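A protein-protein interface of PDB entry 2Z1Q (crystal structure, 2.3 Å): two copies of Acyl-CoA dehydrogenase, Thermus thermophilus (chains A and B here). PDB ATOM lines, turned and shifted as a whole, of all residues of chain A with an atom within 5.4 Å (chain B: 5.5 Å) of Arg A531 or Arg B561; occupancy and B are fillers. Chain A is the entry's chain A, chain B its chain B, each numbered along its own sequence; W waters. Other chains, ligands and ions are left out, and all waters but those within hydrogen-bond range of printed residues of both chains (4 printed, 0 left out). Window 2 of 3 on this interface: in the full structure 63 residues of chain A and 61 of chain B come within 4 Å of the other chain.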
ATOM      1  N   LYS A 467      17.843  21.927  30.635  1.00  0.00           N
ATOM      2  CA  LYS A 467      17.896  20.607  31.237  1.00  0.00           C
ATOM      3  C   LYS A 467      18.855  20.572  32.416  1.00  0.00           C
ATOM      4  O   LYS A 467      18.663  19.810  33.364  1.00  0.00           O
ATOM      5  CB  LYS A 467      18.312  19.589  30.180  1.00  0.00           C
ATOM      6  CG  LYS A 467      18.136  18.136  30.583  1.00  0.00           C
ATOM      7  CD  LYS A 467      19.367  17.591  31.266  1.00  0.00           C
ATOM      8  CE  LYS A 467      19.550  16.099  30.956  1.00  0.00           C
ATOM      9  NZ  LYS A 467      18.437  15.235  31.427  1.00  0.00           N
ATOM     10  N   TYR A 468      19.881  21.408  32.359  1.00  0.00           N
ATOM     11  CA  TYR A 468      20.877  21.464  33.420  1.00  0.00           C
ATOM     12  C   TYR A 468      20.909  22.822  34.106  1.00  0.00           C
ATOM     13  O   TYR A 468      21.494  22.977  35.180  1.00  0.00           O
ATOM     14  CB  TYR A 468      22.247  21.133  32.840  1.00  0.00           C
ATOM     15  CG  TYR A 468      22.391  19.679  32.471  1.00  0.00           C
ATOM     16  CD1 TYR A 468      22.364  18.698  33.457  1.00  0.00           C
ATOM     17  CD2 TYR A 468      22.592  19.282  31.149  1.00  0.00           C
ATOM     18  CE1 TYR A 468      22.544  17.360  33.145  1.00  0.00           C
ATOM     19  CE2 TYR A 468      22.771  17.941  30.824  1.00  0.00           C
ATOM     20  CZ  TYR A 468      22.751  16.985  31.831  1.00  0.00           C
ATOM     21  OH  TYR A 468      22.973  15.658  31.548  1.00  0.00           O
ATOM     22  N   GLU A 474      29.008  21.921  33.971  1.00  0.00           N
ATOM     23  CA  GLU A 474      29.508  20.613  34.375  1.00  0.00           C
ATOM     24  C   GLU A 474      29.499  19.681  33.173  1.00  0.00           C
ATOM     25  O   GLU A 474      30.314  18.769  33.079  1.00  0.00           O
ATOM     26  CB  GLU A 474      28.634  20.026  35.490  1.00  0.00           C
ATOM     27  CG  GLU A 474      28.832  20.685  36.838  1.00  0.00           C
ATOM     28  CD  GLU A 474      30.126  20.258  37.504  1.00  0.00           C
ATOM     29  OE1 GLU A 474      30.193  19.102  37.980  1.00  0.00           O
ATOM     30  OE2 GLU A 474      31.072  21.073  37.550  1.00  0.00           O
ATOM     31  N   GLU A 475      28.573  19.913  32.251  1.00  0.00           N
ATOM     32  CA  GLU A 475      28.479  19.083  31.058  1.00  0.00           C
ATOM     33  C   GLU A 475      29.513  19.514  30.014  1.00  0.00           C
ATOM     34  O   GLU A 475      29.177  19.921  28.903  1.00  0.00           O
ATOM     35  CB  GLU A 475      27.062  19.158  30.482  1.00  0.00           C
ATOM     36  CG  GLU A 475      25.986  18.574  31.407  1.00  0.00           C
ATOM     37  CD  GLU A 475      26.306  17.160  31.882  1.00  0.00           C
ATOM     38  OE1 GLU A 475      26.518  16.276  31.025  1.00  0.00           O
ATOM     39  OE2 GLU A 475      26.336  16.932  33.111  1.00  0.00           O
ATOM     40  N   GLN A 476      30.780  19.396  30.392  1.00  0.00           N
ATOM     41  CA  GLN A 476      31.885  19.785  29.525  1.00  0.00           C
ATOM     42  C   GLN A 476      31.861  19.140  28.148  1.00  0.00           C
ATOM     43  O   GLN A 476      32.154  19.799  27.156  1.00  0.00           O
ATOM     44  CB  GLN A 476      33.209  19.490  30.221  1.00  0.00           C
ATOM     45  CG  GLN A 476      33.414  20.283  31.499  1.00  0.00           C
ATOM     46  CD  GLN A 476      34.818  20.150  32.004  1.00  0.00           C
ATOM     47  OE1 GLN A 476      35.567  19.290  31.538  1.00  0.00           O
ATOM     48  NE2 GLN A 476      35.193  20.987  32.958  1.00  0.00           N
ATOM     49  N   GLU A 477      31.520  17.857  28.079  1.00  0.00           N
ATOM     50  CA  GLU A 477      31.474  17.190  26.784  1.00  0.00           C
ATOM     51  C   GLU A 477      30.418  17.862  25.910  1.00  0.00           C
ATOM     52  O   GLU A 477      30.627  18.029  24.703  1.00  0.00           O
ATOM     53  CB  GLU A 477      31.160  15.695  26.932  1.00  0.00           C
ATOM     54  CG  GLU A 477      32.154  14.919  27.773  1.00  0.00           C
ATOM     55  CD  GLU A 477      31.786  14.888  29.247  1.00  0.00           C
ATOM     56  OE1 GLU A 477      31.484  15.954  29.823  1.00  0.00           O
ATOM     57  OE2 GLU A 477      31.806  13.791  29.831  1.00  0.00           O
ATOM     58  N   VAL A 478      29.297  18.257  26.517  1.00  0.00           N
ATOM     59  CA  VAL A 478      28.219  18.919  25.769  1.00  0.00           C
ATOM     60  C   VAL A 478      28.680  20.275  25.251  1.00  0.00           C
ATOM     61  O   VAL A 478      28.435  20.632  24.092  1.00  0.00           O
ATOM     62  CB  VAL A 478      26.951  19.134  26.644  1.00  0.00           C
ATOM     63  CG1 VAL A 478      25.893  19.909  25.861  1.00  0.00           C
ATOM     64  CG2 VAL A 478      26.380  17.792  27.070  1.00  0.00           C
ATOM     65  N   VAL A 528      25.970  14.023  21.457  1.00  0.00           N
ATOM     66  CA  VAL A 528      25.653  14.675  22.717  1.00  0.00           C
ATOM     67  C   VAL A 528      24.158  14.900  22.945  1.00  0.00           C
ATOM     68  O   VAL A 528      23.711  15.029  24.084  1.00  0.00           O
ATOM     69  CB  VAL A 528      26.401  16.014  22.830  1.00  0.00           C
ATOM     70  CG1 VAL A 528      25.925  16.774  24.040  1.00  0.00           C
ATOM     71  CG2 VAL A 528      27.894  15.755  22.949  1.00  0.00           C
ATOM     72  N   LEU A 529      23.385  14.944  21.867  1.00  0.00           N
ATOM     73  CA  LEU A 529      21.946  15.152  21.983  1.00  0.00           C
ATOM     74  C   LEU A 529      21.259  14.093  22.848  1.00  0.00           C
ATOM     75  O   LEU A 529      20.378  14.415  23.644  1.00  0.00           O
ATOM     76  CB  LEU A 529      21.298  15.197  20.594  1.00  0.00           C
ATOM     77  CG  LEU A 529      21.407  16.540  19.865  1.00  0.00           C
ATOM     78  CD1 LEU A 529      20.810  16.424  18.477  1.00  0.00           C
ATOM     79  CD2 LEU A 529      20.689  17.615  20.670  1.00  0.00           C
ATOM     80  N   PRO A 530      21.649  12.820  22.699  1.00  0.00           N
ATOM     81  CA  PRO A 530      21.025  11.771  23.510  1.00  0.00           C
ATOM     82  C   PRO A 530      21.162  12.039  25.011  1.00  0.00           C
ATOM     83  O   PRO A 530      20.435  11.474  25.826  1.00  0.00           O
ATOM     84  CB  PRO A 530      21.774  10.517  23.076  1.00  0.00           C
ATOM     85  CG  PRO A 530      22.060  10.795  21.638  1.00  0.00           C
ATOM     86  CD  PRO A 530      22.542  12.230  21.685  1.00  0.00           C
ATOM     87  N   ARG A 531      22.101  12.912  25.354  1.00  0.00           N
ATOM     88  CA  ARG A 531      22.381  13.277  26.739  1.00  0.00           C
ATOM     89  C   ARG A 531      21.476  14.419  27.197  1.00  0.00           C
ATOM     90  O   ARG A 531      21.354  14.688  28.394  1.00  0.00           O
ATOM     91  CB  ARG A 531      23.853  13.697  26.845  1.00  0.00           C
ATOM     92  CG  ARG A 531      24.295  14.313  28.166  1.00  0.00           C
ATOM     93  CD  ARG A 531      24.771  13.273  29.174  1.00  0.00           C
ATOM     94  NE  ARG A 531      25.388  13.916  30.335  1.00  0.00           N
ATOM     95  CZ  ARG A 531      25.908  13.265  31.372  1.00  0.00           C
ATOM     96  NH1 ARG A 531      25.898  11.942  31.409  1.00  0.00           N
ATOM     97  NH2 ARG A 531      26.440  13.945  32.380  1.00  0.00           N
ATOM     98  N   LEU A 532      20.836  15.082  26.243  1.00  0.00           N
ATOM     99  CA  LEU A 532      19.970  16.213  26.549  1.00  0.00           C
ATOM    100  C   LEU A 532      18.478  15.921  26.447  1.00  0.00           C
ATOM    101  O   LEU A 532      17.662  16.633  27.033  1.00  0.00           O
ATOM    102  CB  LEU A 532      20.328  17.395  25.642  1.00  0.00           C
ATOM    103  CG  LEU A 532      21.519  18.272  26.052  1.00  0.00           C
ATOM    104  CD1 LEU A 532      22.733  17.424  26.365  1.00  0.00           C
ATOM    105  CD2 LEU A 532      21.831  19.248  24.933  1.00  0.00           C
ATOM    106  N   VAL A 533      18.115  14.880  25.708  1.00  0.00           N
ATOM    107  CA  VAL A 533      16.709  14.537  25.556  1.00  0.00           C
ATOM    108  C   VAL A 533      16.462  13.043  25.410  1.00  0.00           C
ATOM    109  O   VAL A 533      17.381  12.271  25.142  1.00  0.00           O
ATOM    110  CB  VAL A 533      16.086  15.270  24.348  1.00  0.00           C
ATOM    111  CG1 VAL A 533      15.804  16.715  24.716  1.00  0.00           C
ATOM    112  CG2 VAL A 533      17.024  15.214  23.154  1.00  0.00           C
ATOM    113  N   GLY B 300      34.732  16.618  32.749  1.00  0.00           N
ATOM    114  CA  GLY B 300      34.164  15.965  31.589  1.00  0.00           C
ATOM    115  C   GLY B 300      35.109  15.729  30.418  1.00  0.00           C
ATOM    116  O   GLY B 300      35.221  14.608  29.948  1.00  0.00           O
ATOM    117  N   GLN B 303      37.600  13.007  31.021  1.00  0.00           N
ATOM    118  CA  GLN B 303      36.915  11.717  31.032  1.00  0.00           C
ATOM    119  C   GLN B 303      36.625  11.274  29.599  1.00  0.00           C
ATOM    120  O   GLN B 303      36.747  10.097  29.266  1.00  0.00           O
ATOM    121  CB  GLN B 303      35.609  11.795  31.828  1.00  0.00           C
ATOM    122  CG  GLN B 303      35.763  12.206  33.294  1.00  0.00           C
ATOM    123  CD  GLN B 303      34.905  11.355  34.216  1.00  0.00           C
ATOM    124  OE1 GLN B 303      33.754  11.052  33.900  1.00  0.00           O
ATOM    125  NE2 GLN B 303      35.460  10.967  35.362  1.00  0.00           N
ATOM    126  N   ASP B 555      24.389   7.549  23.549  1.00  0.00           N
ATOM    127  CA  ASP B 555      24.865   8.578  24.478  1.00  0.00           C
ATOM    128  C   ASP B 555      26.349   8.367  24.748  1.00  0.00           C
ATOM    129  O   ASP B 555      26.716   7.735  25.744  1.00  0.00           O
ATOM    130  CB  ASP B 555      24.096   8.488  25.796  1.00  0.00           C
ATOM    131  CG  ASP B 555      24.350   9.676  26.714  1.00  0.00           C
ATOM    132  OD1 ASP B 555      25.296  10.459  26.472  1.00  0.00           O
ATOM    133  OD2 ASP B 555      23.592   9.816  27.696  1.00  0.00           O
ATOM    134  N   LEU B 556      27.190   8.893  23.860  1.00  0.00           N
ATOM    135  CA  LEU B 556      28.635   8.746  23.996  1.00  0.00           C
ATOM    136  C   LEU B 556      29.143   9.424  25.259  1.00  0.00           C
ATOM    137  O   LEU B 556      30.109   8.976  25.875  1.00  0.00           O
ATOM    138  CB  LEU B 556      29.339   9.318  22.755  1.00  0.00           C
ATOM    139  CG  LEU B 556      29.010   8.668  21.401  1.00  0.00           C
ATOM    140  CD1 LEU B 556      29.888   9.276  20.309  1.00  0.00           C
ATOM    141  CD2 LEU B 556      29.242   7.168  21.472  1.00  0.00           C
ATOM    142  N   VAL B 557      28.497  10.506  25.659  1.00  0.00           N
ATOM    143  CA  VAL B 557      28.926  11.185  26.859  1.00  0.00           C
ATOM    144  C   VAL B 557      28.840  10.209  28.025  1.00  0.00           C
ATOM    145  O   VAL B 557      29.827   9.992  28.740  1.00  0.00           O
ATOM    146  CB  VAL B 557      28.055  12.391  27.123  1.00  0.00           C
ATOM    147  CG1 VAL B 557      28.592  13.171  28.313  1.00  0.00           C
ATOM    148  CG2 VAL B 557      28.009  13.252  25.875  1.00  0.00           C
ATOM    149  N   ALA B 558      27.666   9.604  28.200  1.00  0.00           N
ATOM    150  CA  ALA B 558      27.444   8.648  29.276  1.00  0.00           C
ATOM    151  C   ALA B 558      28.402   7.472  29.175  1.00  0.00           C
ATOM    152  O   ALA B 558      29.075   7.127  30.141  1.00  0.00           O
ATOM    153  CB  ALA B 558      25.999   8.134  29.244  1.00  0.00           C
ATOM    154  N   LEU B 559      28.468   6.860  28.001  1.00  0.00           N
ATOM    155  CA  LEU B 559      29.328   5.696  27.834  1.00  0.00           C
ATOM    156  C   LEU B 559      30.810   5.985  28.056  1.00  0.00           C
ATOM    157  O   LEU B 559      31.488   5.217  28.737  1.00  0.00           O
ATOM    158  CB  LEU B 559      29.101   5.048  26.456  1.00  0.00           C
ATOM    159  CG  LEU B 559      27.700   4.468  26.185  1.00  0.00           C
ATOM    160  CD1 LEU B 559      27.666   3.826  24.802  1.00  0.00           C
ATOM    161  CD2 LEU B 559      27.349   3.425  27.226  1.00  0.00           C
ATOM    162  N   ARG B 560      31.320   7.079  27.500  1.00  0.00           N
ATOM    163  CA  ARG B 560      32.724   7.391  27.699  1.00  0.00           C
ATOM    164  C   ARG B 560      32.980   7.642  29.177  1.00  0.00           C
ATOM    165  O   ARG B 560      33.963   7.154  29.728  1.00  0.00           O
ATOM    166  CB  ARG B 560      33.135   8.615  26.879  1.00  0.00           C
ATOM    167  CG  ARG B 560      33.220   8.365  25.374  1.00  0.00           C
ATOM    168  CD  ARG B 560      34.117   9.425  24.766  1.00  0.00           C
ATOM    169  NE  ARG B 560      34.201   9.374  23.309  1.00  0.00           N
ATOM    170  CZ  ARG B 560      33.417  10.060  22.477  1.00  0.00           C
ATOM    171  NH1 ARG B 560      32.468  10.865  22.942  1.00  0.00           N
ATOM    172  NH2 ARG B 560      33.597   9.958  21.170  1.00  0.00           N
ATOM    173  N   ARG B 561      32.085   8.375  29.837  1.00  0.00           N
ATOM    174  CA  ARG B 561      32.271   8.639  31.262  1.00  0.00           C
ATOM    175  C   ARG B 561      32.340   7.342  32.056  1.00  0.00           C
ATOM    176  O   ARG B 561      33.100   7.233  33.019  1.00  0.00           O
ATOM    177  CB  ARG B 561      31.159   9.519  31.816  1.00  0.00           C
ATOM    178  CG  ARG B 561      31.277  10.975  31.411  1.00  0.00           C
ATOM    179  CD  ARG B 561      30.425  11.840  32.313  1.00  0.00           C
ATOM    180  NE  ARG B 561      30.578  13.258  32.013  1.00  0.00           N
ATOM    181  CZ  ARG B 561      30.153  14.231  32.811  1.00  0.00           C
ATOM    182  NH1 ARG B 561      29.552  13.928  33.953  1.00  0.00           N
ATOM    183  NH2 ARG B 561      30.324  15.501  32.470  1.00  0.00           N
ATOM    184  N   GLN B 562      31.547   6.359  31.638  1.00  0.00           N
ATOM    185  CA  GLN B 562      31.512   5.055  32.295  1.00  0.00           C
ATOM    186  C   GLN B 562      32.872   4.349  32.147  1.00  0.00           C
ATOM    187  O   GLN B 562      33.376   3.748  33.097  1.00  0.00           O
ATOM    188  CB  GLN B 562      30.382   4.203  31.694  1.00  0.00           C
ATOM    189  CG  GLN B 562      30.248   2.814  32.300  1.00  0.00           C
ATOM    190  CD  GLN B 562      29.050   2.027  31.754  1.00  0.00           C
ATOM    191  OE1 GLN B 562      28.900   0.841  32.041  1.00  0.00           O
ATOM    192  NE2 GLN B 562      28.198   2.686  30.971  1.00  0.00           N
ATOM    193  N   ALA B 563      33.449   4.436  30.949  1.00  0.00           N
ATOM    194  CA  ALA B 563      34.754   3.836  30.654  1.00  0.00           C
ATOM    195  C   ALA B 563      35.845   4.567  31.449  1.00  0.00           C
ATOM    196  O   ALA B 563      36.730   3.941  32.035  1.00  0.00           O
ATOM    197  CB  ALA B 563      35.037   3.930  29.151  1.00  0.00           C
ATOM    198  N   ALA B 564      35.755   5.895  31.456  1.00  0.00           N
ATOM    199  CA  ALA B 564      36.693   6.748  32.187  1.00  0.00           C
ATOM    200  C   ALA B 564      36.759   6.293  33.637  1.00  0.00           C
ATOM    201  O   ALA B 564      37.830   5.952  34.140  1.00  0.00           O
ATOM    202  CB  ALA B 564      36.234   8.214  32.118  1.00  0.00           C
ATOM    203  N   GLU B 565      35.607   6.284  34.304  1.00  0.00           N
ATOM    204  CA  GLU B 565      35.538   5.857  35.697  1.00  0.00           C
ATOM    205  C   GLU B 565      36.286   4.538  35.880  1.00  0.00           C
ATOM    206  O   GLU B 565      37.067   4.383  36.825  1.00  0.00           O
ATOM    207  CB  GLU B 565      34.078   5.703  36.141  1.00  0.00           C
ATOM    208  CG  GLU B 565      33.293   7.024  36.239  1.00  0.00           C
ATOM    209  CD  GLU B 565      33.933   8.017  37.206  1.00  0.00           C
ATOM    210  OE1 GLU B 565      34.773   7.591  38.030  1.00  0.00           O
ATOM    211  OE2 GLU B 565      33.590   9.220  37.150  1.00  0.00           O
ATOM    212  N   ALA B 566      36.064   3.599  34.965  1.00  0.00           N
ATOM    213  CA  ALA B 566      36.731   2.302  35.031  1.00  0.00           C
ATOM    214  C   ALA B 566      38.244   2.454  34.839  1.00  0.00           C
ATOM    215  O   ALA B 566      39.034   1.735  35.456  1.00  0.00           O
ATOM    216  CB  ALA B 566      36.168   1.369  33.969  1.00  0.00           C
HETATM  217  O   HOH W   1      32.133  11.548  27.904  1.00  0.00           O
HETATM  218  O   HOH W   2      23.359  10.298  30.376  1.00  0.00           O
HETATM  219  O   HOH W   3      32.638  18.020  34.375  1.00  0.00           O
HETATM  220  O   HOH W   4      24.983  12.139  24.397  1.00  0.00           O
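The guanidinium group (NE) of Arg B561 is in salt-bridge range of the side-chain carboxylate (OE2) of Glu A477 (2.6 Å). OE1 of Gln A476 lies within hydrogen-bond range of N of Gly B300, 3.1 Å away. The guanidinium group of Arg B561 is in hydrogen-bond range of the backbone carbonyl oxygen of Glu A474, 3.3 Å away. NH2 of Arg A531 lies close to NH1 of Arg B561.
The backbone NH (N) of Val B557 sits close to the side-chain carboxylate (OD1) of Asp B555 (3.3 Å). The side-chain carboxylate of Glu A475 is in salt-bridge range of the guanidinium group of Arg A531, at 2.7 Å. The side-chain hydroxyl (OH) of Tyr A468 sits at hydrogen-bond distance from the guanidinium group (NE) of Arg A531, at 3.2 Å. The side-chain carboxylate of Asp B555 lies within hydrogen-bond range of the backbone NH of Ala B558 (3.1 Å).
OE1 of Glu A477 touches CA of Gly B300, at 3.2 Å. CG1 of Val B557 touches OE2 of Glu A477, 3.6 Å away. Val A528 touches Val B557 (CG2 to CG2, 3.9 Å). Pro A530 touches Asp B555. Arg A531 touches Asp B555 (CB to OD1, 3.6 Å). Arg A531 touches Val B557.
Lys A467 touches none of the printed residues of chain B. Of the printed residues of chain B, Gln A476 touches Gly B300. Val A478 touches none of the printed residues of chain B. Printed residues of chain A within 4 Å of Asp B555: Pro A530 and Arg A531. Of chain A, only Glu A474 (3.3 Å), Glu A477 (2.6 Å) and Arg A531 (3.5 Å) come within 4 Å of Arg B561.
Printed residues of chain B that touch a printed residue of chain A: Gly B300, Asp B555, Val B557 and Arg B561. Hydrophobic or aromatic side chains of chain B that line the printed part of chain A: Val B557. Printed residues of chain A that touch a printed residue of chain B: Glu A474, Gln A476, Glu A477, Val A528, Pro A530 and Arg A531. Hydrophobic or aromatic side chains of chain A that line the printed part of chain B: Val A528 and Pro A530. Along chain A the printed residues that touch a printed residue of chain B span positions 474 to 531.
No position is printed for both chains. Of the 10 pairs that touch across the chains among the printed residues, none has its exchanged pair printed and touching as well.
Water W4 lies within hydrogen-bond range of OD1 of Asp B555 (2.7 Å), N of Arg A531 (3.1 Å) and O of Val A528 (3.2 Å). Water W2 bridges the side-chain carboxylate of Asp B555 (2.7 Å) and the guanidinium group of Arg A531 (3.2 Å). Water W3 lies within hydrogen-bond range of O of Glu A474 (2.8 Å) and N of Gly B300 (3.0 Å). Water W1 bridges O of Val B557 and OE2 of Glu A477.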
